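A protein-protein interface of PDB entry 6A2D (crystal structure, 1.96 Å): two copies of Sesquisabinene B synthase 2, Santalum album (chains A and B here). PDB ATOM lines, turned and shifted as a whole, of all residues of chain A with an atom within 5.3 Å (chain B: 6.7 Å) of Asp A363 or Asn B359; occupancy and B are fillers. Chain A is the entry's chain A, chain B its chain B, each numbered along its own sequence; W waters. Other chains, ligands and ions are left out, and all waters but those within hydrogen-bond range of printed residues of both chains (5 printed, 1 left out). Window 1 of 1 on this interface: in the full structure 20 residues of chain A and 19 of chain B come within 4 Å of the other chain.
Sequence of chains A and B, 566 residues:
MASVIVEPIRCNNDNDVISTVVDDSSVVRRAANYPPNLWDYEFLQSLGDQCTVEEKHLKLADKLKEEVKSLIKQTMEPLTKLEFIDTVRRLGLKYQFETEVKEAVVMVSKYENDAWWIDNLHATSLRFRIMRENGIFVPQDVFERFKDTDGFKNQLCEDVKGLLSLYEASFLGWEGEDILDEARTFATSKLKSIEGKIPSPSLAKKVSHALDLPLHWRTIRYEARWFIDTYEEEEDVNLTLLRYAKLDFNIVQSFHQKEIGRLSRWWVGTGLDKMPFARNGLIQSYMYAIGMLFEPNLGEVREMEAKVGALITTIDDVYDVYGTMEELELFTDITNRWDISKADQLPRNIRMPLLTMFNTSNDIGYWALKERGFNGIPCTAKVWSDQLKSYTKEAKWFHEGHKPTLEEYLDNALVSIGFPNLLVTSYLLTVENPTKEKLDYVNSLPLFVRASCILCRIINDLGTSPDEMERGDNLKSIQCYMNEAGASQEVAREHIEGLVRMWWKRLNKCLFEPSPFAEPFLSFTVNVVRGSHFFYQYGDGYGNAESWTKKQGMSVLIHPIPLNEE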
ATOM      1  N   LYS A 307      -8.620 -15.463 -20.432  1.00  0.00           N
ATOM      2  CA  LYS A 307      -9.842 -15.902 -19.715  1.00  0.00           C
ATOM      3  C   LYS A 307     -10.547 -16.973 -20.541  1.00  0.00           C
ATOM      4  O   LYS A 307     -10.868 -18.027 -19.998  1.00  0.00           O
ATOM      5  CB  LYS A 307     -10.831 -14.769 -19.485  1.00  0.00           C
ATOM      6  CG  LYS A 307     -10.370 -13.737 -18.480  1.00  0.00           C
ATOM      7  CD  LYS A 307     -11.474 -12.751 -18.223  1.00  0.00           C
ATOM      8  CE  LYS A 307     -11.112 -11.767 -17.146  1.00  0.00           C
ATOM      9  NZ  LYS A 307     -12.296 -10.935 -16.884  1.00  0.00           N
ATOM     10  N   PHE A 358     -20.575 -18.717 -18.944  1.00  0.00           N
ATOM     11  CA  PHE A 358     -21.726 -17.849 -19.249  1.00  0.00           C
ATOM     12  C   PHE A 358     -21.380 -16.391 -18.908  1.00  0.00           C
ATOM     13  O   PHE A 358     -21.462 -15.566 -19.780  1.00  0.00           O
ATOM     14  CB  PHE A 358     -22.962 -18.358 -18.507  1.00  0.00           C
ATOM     15  CG  PHE A 358     -24.221 -17.579 -18.722  1.00  0.00           C
ATOM     16  CD1 PHE A 358     -24.963 -17.745 -19.876  1.00  0.00           C
ATOM     17  CD2 PHE A 358     -24.697 -16.723 -17.753  1.00  0.00           C
ATOM     18  CE1 PHE A 358     -26.155 -17.051 -20.054  1.00  0.00           C
ATOM     19  CE2 PHE A 358     -25.893 -16.040 -17.925  1.00  0.00           C
ATOM     20  CZ  PHE A 358     -26.643 -16.240 -19.050  1.00  0.00           C
ATOM     21  N   ASN A 359     -20.930 -16.138 -17.689  1.00  0.00           N
ATOM     22  CA  ASN A 359     -20.666 -14.773 -17.170  1.00  0.00           C
ATOM     23  C   ASN A 359     -19.509 -14.131 -17.954  1.00  0.00           C
ATOM     24  O   ASN A 359     -19.619 -12.948 -18.303  1.00  0.00           O
ATOM     25  CB  ASN A 359     -20.419 -14.778 -15.677  1.00  0.00           C
ATOM     26  CG  ASN A 359     -21.658 -15.075 -14.870  1.00  0.00           C
ATOM     27  OD1 ASN A 359     -22.759 -15.153 -15.403  1.00  0.00           O
ATOM     28  ND2 ASN A 359     -21.488 -15.221 -13.571  1.00  0.00           N
ATOM     29  N   THR A 360     -18.461 -14.893 -18.256  1.00  0.00           N
ATOM     30  CA  THR A 360     -17.281 -14.380 -18.962  1.00  0.00           C
ATOM     31  C   THR A 360     -17.628 -14.096 -20.420  1.00  0.00           C
ATOM     32  O   THR A 360     -17.233 -12.996 -20.957  1.00  0.00           O
ATOM     33  CB  THR A 360     -16.111 -15.344 -18.823  1.00  0.00           C
ATOM     34  OG1 THR A 360     -15.708 -15.323 -17.468  1.00  0.00           O
ATOM     35  CG2 THR A 360     -14.953 -14.950 -19.702  1.00  0.00           C
ATOM     36  N   SER A 361     -18.383 -14.978 -21.054  1.00  0.00           N
ATOM     37  CA  SER A 361     -18.854 -14.770 -22.440  1.00  0.00           C
ATOM     38  C   SER A 361     -19.723 -13.499 -22.533  1.00  0.00           C
ATOM     39  O   SER A 361     -19.524 -12.748 -23.484  1.00  0.00           O
ATOM     40  CB  SER A 361     -19.582 -15.953 -22.962  1.00  0.00           C
ATOM     41  OG  SER A 361     -18.679 -17.058 -23.020  1.00  0.00           O
ATOM     42  N   ASN A 362     -20.616 -13.278 -21.576  1.00  0.00           N
ATOM     43  CA  ASN A 362     -21.441 -12.051 -21.491  1.00  0.00           C
ATOM     44  C   ASN A 362     -20.526 -10.834 -21.303  1.00  0.00           C
ATOM     45  O   ASN A 362     -20.796  -9.859 -21.962  1.00  0.00           O
ATOM     46  CB  ASN A 362     -22.512 -12.148 -20.423  1.00  0.00           C
ATOM     47  CG  ASN A 362     -23.535 -13.189 -20.784  1.00  0.00           C
ATOM     48  OD1 ASN A 362     -23.707 -13.495 -21.967  1.00  0.00           O
ATOM     49  ND2 ASN A 362     -24.175 -13.767 -19.779  1.00  0.00           N
ATOM     50  N   ASP A 363     -19.501 -10.903 -20.447  1.00  0.00           N
ATOM     51  CA  ASP A 363     -18.569  -9.785 -20.201  1.00  0.00           C
ATOM     52  C   ASP A 363     -17.804  -9.469 -21.493  1.00  0.00           C
ATOM     53  O   ASP A 363     -17.643  -8.284 -21.828  1.00  0.00           O
ATOM     54  CB  ASP A 363     -17.536 -10.080 -19.127  1.00  0.00           C
ATOM     55  CG  ASP A 363     -18.063 -10.118 -17.696  1.00  0.00           C
ATOM     56  OD1 ASP A 363     -19.207  -9.656 -17.459  1.00  0.00           O
ATOM     57  OD2 ASP A 363     -17.327 -10.666 -16.830  1.00  0.00           O
ATOM     58  N   ILE A 364     -17.319 -10.486 -22.175  1.00  0.00           N
ATOM     59  CA  ILE A 364     -16.534 -10.296 -23.429  1.00  0.00           C
ATOM     60  C   ILE A 364     -17.435  -9.688 -24.508  1.00  0.00           C
ATOM     61  O   ILE A 364     -17.013  -8.696 -25.126  1.00  0.00           O
ATOM     62  CB  ILE A 364     -15.818 -11.589 -23.853  1.00  0.00           C
ATOM     63  CG1 ILE A 364     -14.737 -11.963 -22.840  1.00  0.00           C
ATOM     64  CG2 ILE A 364     -15.235 -11.393 -25.221  1.00  0.00           C
ATOM     65  CD1 ILE A 364     -14.092 -13.318 -23.051  1.00  0.00           C
ATOM     66  N   GLY A 365     -18.624 -10.235 -24.718  1.00  0.00           N
ATOM     67  CA  GLY A 365     -19.616  -9.682 -25.650  1.00  0.00           C
ATOM     68  C   GLY A 365     -19.923  -8.220 -25.328  1.00  0.00           C
ATOM     69  O   GLY A 365     -20.058  -7.374 -26.291  1.00  0.00           O
ATOM     70  N   TYR A 366     -20.037  -7.917 -24.032  1.00  0.00           N
ATOM     71  CA  TYR A 366     -20.375  -6.569 -23.539  1.00  0.00           C
ATOM     72  C   TYR A 366     -19.207  -5.624 -23.830  1.00  0.00           C
ATOM     73  O   TYR A 366     -19.457  -4.501 -24.256  1.00  0.00           O
ATOM     74  CB  TYR A 366     -20.770  -6.575 -22.066  1.00  0.00           C
ATOM     75  CG  TYR A 366     -21.183  -5.210 -21.612  1.00  0.00           C
ATOM     76  CD1 TYR A 366     -20.241  -4.293 -21.215  1.00  0.00           C
ATOM     77  CD2 TYR A 366     -22.505  -4.814 -21.655  1.00  0.00           C
ATOM     78  CE1 TYR A 366     -20.607  -3.034 -20.795  1.00  0.00           C
ATOM     79  CE2 TYR A 366     -22.887  -3.546 -21.262  1.00  0.00           C
ATOM     80  CZ  TYR A 366     -21.928  -2.647 -20.852  1.00  0.00           C
ATOM     81  OH  TYR A 366     -22.238  -1.375 -20.476  1.00  0.00           O
ATOM     82  N   TRP A 367     -17.969  -6.060 -23.645  1.00  0.00           N
ATOM     83  CA  TRP A 367     -16.801  -5.221 -23.979  1.00  0.00           C
ATOM     84  C   TRP A 367     -16.895  -4.762 -25.435  1.00  0.00           C
ATOM     85  O   TRP A 367     -16.674  -3.554 -25.676  1.00  0.00           O
ATOM     86  CB  TRP A 367     -15.512  -5.969 -23.717  1.00  0.00           C
ATOM     87  CG  TRP A 367     -14.287  -5.134 -23.831  1.00  0.00           C
ATOM     88  CD1 TRP A 367     -13.574  -4.603 -22.802  1.00  0.00           C
ATOM     89  CD2 TRP A 367     -13.529  -4.885 -25.024  1.00  0.00           C
ATOM     90  NE1 TRP A 367     -12.424  -4.034 -23.273  1.00  0.00           N
ATOM     91  CE2 TRP A 367     -12.399  -4.148 -24.646  1.00  0.00           C
ATOM     92  CE3 TRP A 367     -13.706  -5.187 -26.365  1.00  0.00           C
ATOM     93  CZ2 TRP A 367     -11.431  -3.742 -25.567  1.00  0.00           C
ATOM     94  CZ3 TRP A 367     -12.782  -4.749 -27.282  1.00  0.00           C
ATOM     95  CH2 TRP A 367     -11.660  -4.034 -26.886  1.00  0.00           C
ATOM     96  N   ALA A 368     -17.223  -5.666 -26.366  1.00  0.00           N
ATOM     97  CA  ALA A 368     -17.353  -5.325 -27.798  1.00  0.00           C
ATOM     98  C   ALA A 368     -18.419  -4.235 -27.957  1.00  0.00           C
ATOM     99  O   ALA A 368     -18.253  -3.357 -28.816  1.00  0.00           O
ATOM    100  CB  ALA A 368     -17.686  -6.543 -28.629  1.00  0.00           C
ATOM    101  N   ILE A 377     -22.254 -10.672 -27.622  1.00  0.00           N
ATOM    102  CA  ILE A 377     -22.774 -11.832 -26.845  1.00  0.00           C
ATOM    103  C   ILE A 377     -23.261 -12.920 -27.794  1.00  0.00           C
ATOM    104  O   ILE A 377     -22.934 -14.107 -27.588  1.00  0.00           O
ATOM    105  CB  ILE A 377     -23.796 -11.416 -25.771  1.00  0.00           C
ATOM    106  CG1 ILE A 377     -23.074 -10.571 -24.728  1.00  0.00           C
ATOM    107  CG2 ILE A 377     -24.486 -12.649 -25.175  1.00  0.00           C
ATOM    108  CD1 ILE A 377     -23.931  -9.962 -23.656  1.00  0.00           C
ATOM    109  N   TRP B 338     -35.245 -12.769 -17.616  1.00  0.00           N
ATOM    110  CA  TRP B 338     -33.771 -12.993 -17.564  1.00  0.00           C
ATOM    111  C   TRP B 338     -33.301 -13.593 -18.885  1.00  0.00           C
ATOM    112  O   TRP B 338     -32.624 -14.617 -18.877  1.00  0.00           O
ATOM    113  CB  TRP B 338     -33.373 -13.878 -16.390  1.00  0.00           C
ATOM    114  CG  TRP B 338     -32.060 -13.490 -15.770  1.00  0.00           C
ATOM    115  CD1 TRP B 338     -30.942 -14.264 -15.621  1.00  0.00           C
ATOM    116  CD2 TRP B 338     -31.756 -12.224 -15.168  1.00  0.00           C
ATOM    117  NE1 TRP B 338     -29.971 -13.578 -14.933  1.00  0.00           N
ATOM    118  CE2 TRP B 338     -30.446 -12.321 -14.643  1.00  0.00           C
ATOM    119  CE3 TRP B 338     -32.475 -11.039 -14.981  1.00  0.00           C
ATOM    120  CZ2 TRP B 338     -29.833 -11.247 -14.001  1.00  0.00           C
ATOM    121  CZ3 TRP B 338     -31.871  -9.985 -14.329  1.00  0.00           C
ATOM    122  CH2 TRP B 338     -30.569 -10.091 -13.845  1.00  0.00           C
ATOM    123  N   ILE B 340     -31.785 -12.073 -22.540  1.00  0.00           N
ATOM    124  CA  ILE B 340     -31.198 -10.877 -23.213  1.00  0.00           C
ATOM    125  C   ILE B 340     -31.198 -11.065 -24.736  1.00  0.00           C
ATOM    126  O   ILE B 340     -30.551 -10.271 -25.409  1.00  0.00           O
ATOM    127  CB  ILE B 340     -29.787 -10.616 -22.666  1.00  0.00           C
ATOM    128  CG1 ILE B 340     -28.835 -11.778 -22.939  1.00  0.00           C
ATOM    129  CG2 ILE B 340     -29.837 -10.286 -21.182  1.00  0.00           C
ATOM    130  CD1 ILE B 340     -27.376 -11.417 -22.736  1.00  0.00           C
ATOM    131  N   LEU B 354     -28.746  -2.034 -19.118  1.00  0.00           N
ATOM    132  CA  LEU B 354     -29.487  -3.312 -19.052  1.00  0.00           C
ATOM    133  C   LEU B 354     -28.494  -4.473 -18.942  1.00  0.00           C
ATOM    134  O   LEU B 354     -28.673  -5.305 -18.062  1.00  0.00           O
ATOM    135  CB  LEU B 354     -30.340  -3.504 -20.303  1.00  0.00           C
ATOM    136  CG  LEU B 354     -30.964  -4.894 -20.408  1.00  0.00           C
ATOM    137  CD1 LEU B 354     -32.103  -5.027 -19.417  1.00  0.00           C
ATOM    138  CD2 LEU B 354     -31.444  -5.196 -21.813  1.00  0.00           C
ATOM    139  N   LEU B 355     -27.514  -4.543 -19.841  1.00  0.00           N
ATOM    140  CA  LEU B 355     -26.601  -5.712 -19.912  1.00  0.00           C
ATOM    141  C   LEU B 355     -25.664  -5.642 -18.736  1.00  0.00           C
ATOM    142  O   LEU B 355     -25.267  -6.711 -18.232  1.00  0.00           O
ATOM    143  CB  LEU B 355     -25.872  -5.750 -21.254  1.00  0.00           C
ATOM    144  CG  LEU B 355     -26.776  -6.126 -22.422  1.00  0.00           C
ATOM    145  CD1 LEU B 355     -26.054  -5.971 -23.739  1.00  0.00           C
ATOM    146  CD2 LEU B 355     -27.326  -7.545 -22.259  1.00  0.00           C
ATOM    147  N   THR B 356     -25.382  -4.437 -18.238  1.00  0.00           N
ATOM    148  CA  THR B 356     -24.525  -4.285 -17.047  1.00  0.00           C
ATOM    149  C   THR B 356     -25.315  -4.774 -15.837  1.00  0.00           C
ATOM    150  O   THR B 356     -24.728  -5.421 -14.988  1.00  0.00           O
ATOM    151  CB  THR B 356     -23.962  -2.869 -16.886  1.00  0.00           C
ATOM    152  OG1 THR B 356     -23.050  -2.581 -17.964  1.00  0.00           O
ATOM    153  CG2 THR B 356     -23.212  -2.746 -15.585  1.00  0.00           C
ATOM    154  N   MET B 357     -26.610  -4.484 -15.771  1.00  0.00           N
ATOM    155  CA  MET B 357     -27.451  -4.935 -14.644  1.00  0.00           C
ATOM    156  C   MET B 357     -27.469  -6.471 -14.662  1.00  0.00           C
ATOM    157  O   MET B 357     -27.364  -7.076 -13.591  1.00  0.00           O
ATOM    158  CB  MET B 357     -28.878  -4.383 -14.752  1.00  0.00           C
ATOM    159  CG  MET B 357     -29.855  -5.005 -13.759  1.00  0.00           C
ATOM    160  SD  MET B 357     -31.541  -5.035 -14.435  1.00  0.00           S
ATOM    161  CE  MET B 357     -31.401  -6.357 -15.640  1.00  0.00           C
ATOM    162  N   PHE B 358     -27.725  -7.033 -15.817  1.00  0.00           N
ATOM    163  CA  PHE B 358     -27.744  -8.498 -16.063  1.00  0.00           C
ATOM    164  C   PHE B 358     -26.396  -9.104 -15.668  1.00  0.00           C
ATOM    165  O   PHE B 358     -26.377 -10.004 -14.855  1.00  0.00           O
ATOM    166  CB  PHE B 358     -28.103  -8.737 -17.521  1.00  0.00           C
ATOM    167  CG  PHE B 358     -28.223 -10.168 -17.939  1.00  0.00           C
ATOM    168  CD1 PHE B 358     -29.337 -10.911 -17.601  1.00  0.00           C
ATOM    169  CD2 PHE B 358     -27.227 -10.763 -18.698  1.00  0.00           C
ATOM    170  CE1 PHE B 358     -29.468 -12.218 -18.021  1.00  0.00           C
ATOM    171  CE2 PHE B 358     -27.353 -12.080 -19.106  1.00  0.00           C
ATOM    172  CZ  PHE B 358     -28.492 -12.792 -18.801  1.00  0.00           C
ATOM    173  N   ASN B 359     -25.296  -8.569 -16.193  1.00  0.00           N
ATOM    174  CA  ASN B 359     -23.943  -9.126 -15.957  1.00  0.00           C
ATOM    175  C   ASN B 359     -23.572  -9.039 -14.486  1.00  0.00           C
ATOM    176  O   ASN B 359     -23.119 -10.080 -13.932  1.00  0.00           O
ATOM    177  CB  ASN B 359     -22.880  -8.503 -16.839  1.00  0.00           C
ATOM    178  CG  ASN B 359     -23.046  -8.858 -18.289  1.00  0.00           C
ATOM    179  OD1 ASN B 359     -23.793  -9.754 -18.623  1.00  0.00           O
ATOM    180  ND2 ASN B 359     -22.363  -8.137 -19.167  1.00  0.00           N
ATOM    181  N   THR B 360     -23.818  -7.902 -13.839  1.00  0.00           N
ATOM    182  CA  THR B 360     -23.505  -7.688 -12.413  1.00  0.00           C
ATOM    183  C   THR B 360     -24.379  -8.589 -11.529  1.00  0.00           C
ATOM    184  O   THR B 360     -23.846  -9.188 -10.590  1.00  0.00           O
ATOM    185  CB  THR B 360     -23.589  -6.190 -12.074  1.00  0.00           C
ATOM    186  OG1 THR B 360     -22.520  -5.510 -12.739  1.00  0.00           O
ATOM    187  CG2 THR B 360     -23.501  -5.930 -10.595  1.00  0.00           C
ATOM    188  N   SER B 361     -25.663  -8.735 -11.832  1.00  0.00           N
ATOM    189  CA  SER B 361     -26.580  -9.606 -11.073  1.00  0.00           C
ATOM    190  C   SER B 361     -26.084 -11.062 -11.167  1.00  0.00           C
ATOM    191  O   SER B 361     -26.160 -11.764 -10.177  1.00  0.00           O
ATOM    192  CB  SER B 361     -27.984  -9.483 -11.595  1.00  0.00           C
ATOM    193  OG  SER B 361     -28.494  -8.183 -11.395  1.00  0.00           O
ATOM    194  N   ASN B 362     -25.659 -11.484 -12.358  1.00  0.00           N
ATOM    195  CA  ASN B 362     -25.119 -12.834 -12.589  1.00  0.00           C
ATOM    196  C   ASN B 362     -23.839 -12.966 -11.789  1.00  0.00           C
ATOM    197  O   ASN B 362     -23.675 -14.006 -11.137  1.00  0.00           O
ATOM    198  CB  ASN B 362     -24.949 -13.115 -14.066  1.00  0.00           C
ATOM    199  CG  ASN B 362     -26.257 -13.258 -14.794  1.00  0.00           C
ATOM    200  OD1 ASN B 362     -27.266 -13.626 -14.195  1.00  0.00           O
ATOM    201  ND2 ASN B 362     -26.232 -13.011 -16.095  1.00  0.00           N
ATOM    202  N   ASP B 363     -22.985 -11.946 -11.769  1.00  0.00           N
ATOM    203  CA  ASP B 363     -21.737 -12.013 -10.981  1.00  0.00           C
ATOM    204  C   ASP B 363     -22.080 -12.159  -9.501  1.00  0.00           C
ATOM    205  O   ASP B 363     -21.413 -12.897  -8.813  1.00  0.00           O
ATOM    206  CB  ASP B 363     -20.833 -10.792 -11.153  1.00  0.00           C
ATOM    207  CG  ASP B 363     -20.138 -10.688 -12.507  1.00  0.00           C
ATOM    208  OD1 ASP B 363     -20.026 -11.723 -13.210  1.00  0.00           O
ATOM    209  OD2 ASP B 363     -19.773  -9.571 -12.854  1.00  0.00           O
ATOM    210  N   ILE B 364     -23.007 -11.370  -8.989  1.00  0.00           N
ATOM    211  CA  ILE B 364     -23.274 -11.356  -7.517  1.00  0.00           C
ATOM    212  C   ILE B 364     -23.924 -12.693  -7.127  1.00  0.00           C
ATOM    213  O   ILE B 364     -23.516 -13.292  -6.126  1.00  0.00           O
ATOM    214  CB  ILE B 364     -24.131 -10.126  -7.175  1.00  0.00           C
ATOM    215  CG1 ILE B 364     -23.314  -8.838  -7.299  1.00  0.00           C
ATOM    216  CG2 ILE B 364     -24.790 -10.276  -5.796  1.00  0.00           C
ATOM    217  CD1 ILE B 364     -24.169  -7.585  -7.230  1.00  0.00           C
HETATM  218  O   HOH W   1     -19.675  -8.329 -15.189  1.00  0.00           O
HETATM  219  O   HOH W   2     -17.958 -12.201 -14.765  1.00  0.00           O
HETATM  220  O   HOH W   3     -19.515  -6.841 -18.430  1.00  0.00           O
HETATM  221  O   HOH W   4     -18.987 -14.095 -12.081  1.00  0.00           O
HETATM  222  O   HOH W   5     -23.539 -12.527 -17.151  1.00  0.00           O
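The side-chain amide nitrogen (ND2) of Asn A359 lies within hydrogen-bond range of the backbone carbonyl oxygen (O) of Asn B362.
The side-chain hydroxyl of Tyr A366 lies within hydrogen-bond range of the side-chain hydroxyl of Thr B356.
O of Phe A358 is in hydrogen-bond range of ND2 of Asn A362 (3.3 Å).
The indole nitrogen (NE1) of Trp B338 is in hydrogen-bond range of the side-chain amide oxygen (OD1) of Asn B362.
O of Leu B355 lies close to ND2 of Asn B359, 3.4 Å away.
O of Thr B356 sits at hydrogen-bond distance from OG1 of Thr B360 (3.2 Å).
ND2 of Asn B362 lies within hydrogen-bond range of O of Phe B358.
Among the printed residues, merely in contact across the chains: Phe A358 with Phe B358 (3.9 Å), Phe A358 with Asn B362 (3.6 Å), Asn A359 with Asp B363 (3.8 Å), Asn A362 with Phe B358 (3.7 Å), Asn A362 with Asn B359 (3.3 Å), Asp A363 with Asn B359 (3.9 Å), Tyr A366 with Leu B355 (3.5 Å), Tyr A366 with Asn B359 (3.7 Å) and Ile A377 with Ile B340 (3.9 Å).
Asn B359 touches just these residues of chain A: Asn A362, Asp A363 and Tyr A366.
Printed residues of chain A within 4 Å of Leu B355: Tyr A366.
Printed residues of chain A within 4 Å of Phe B358: Phe A358 and Asn A362.
The nearest residue of chain B that does not touch Asp A363 is Asp B363 (4.6 Å).
The nearest residue of chain A that does not touch Asn B359 is Ile A377 (5.0 Å).
The nearest printed residue of chain A that does not touch Asp B363 is Asp A363 (4.6 Å).
Of the 13 printed residues of chain A, 6 touch a printed residue of chain B.
Among the printed residues, 11 pairs touch across the chains.
Phe B358 touches its own counterpart, Phe A358.
Phe A358 touches Asn B362, and with the chains exchanged Asn A362 touches Phe B358.
Asn A359 touches Asn B362, and with the chains exchanged Asn A362 touches Asn B359.
Asn A359 touches Asp B363, and with the chains exchanged Asp A363 touches Asn B359.
Positions printed for both chains: 358, 359, 360, 361, 362, 363 and 364.
Of the 11 pairs that touch across the chains among the printed residues, 7 have their exchanged pair printed and touching as well.
Water W2 lies within hydrogen-bond range of OD1 of Asp B363 (2.6 Å) and OD2 of Asp A363 (2.6 Å).
Water W1 lies within hydrogen-bond range of the side-chain carboxylate of Asp B363 and the side-chain carboxylate of Asp A363.
Water W4 bridges OD1 of Asp B363 (2.8 Å) and ND2 of Asn A359 (3.1 Å).
Water W5 lies within hydrogen-bond range of ND2 of Asn B362, ND2 of Asn A362, OD1 of Asn B359 and OD1 of Asn A359.
Water W3 lies within hydrogen-bond range of OD1 of Asp A363 and ND2 of Asn B359.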
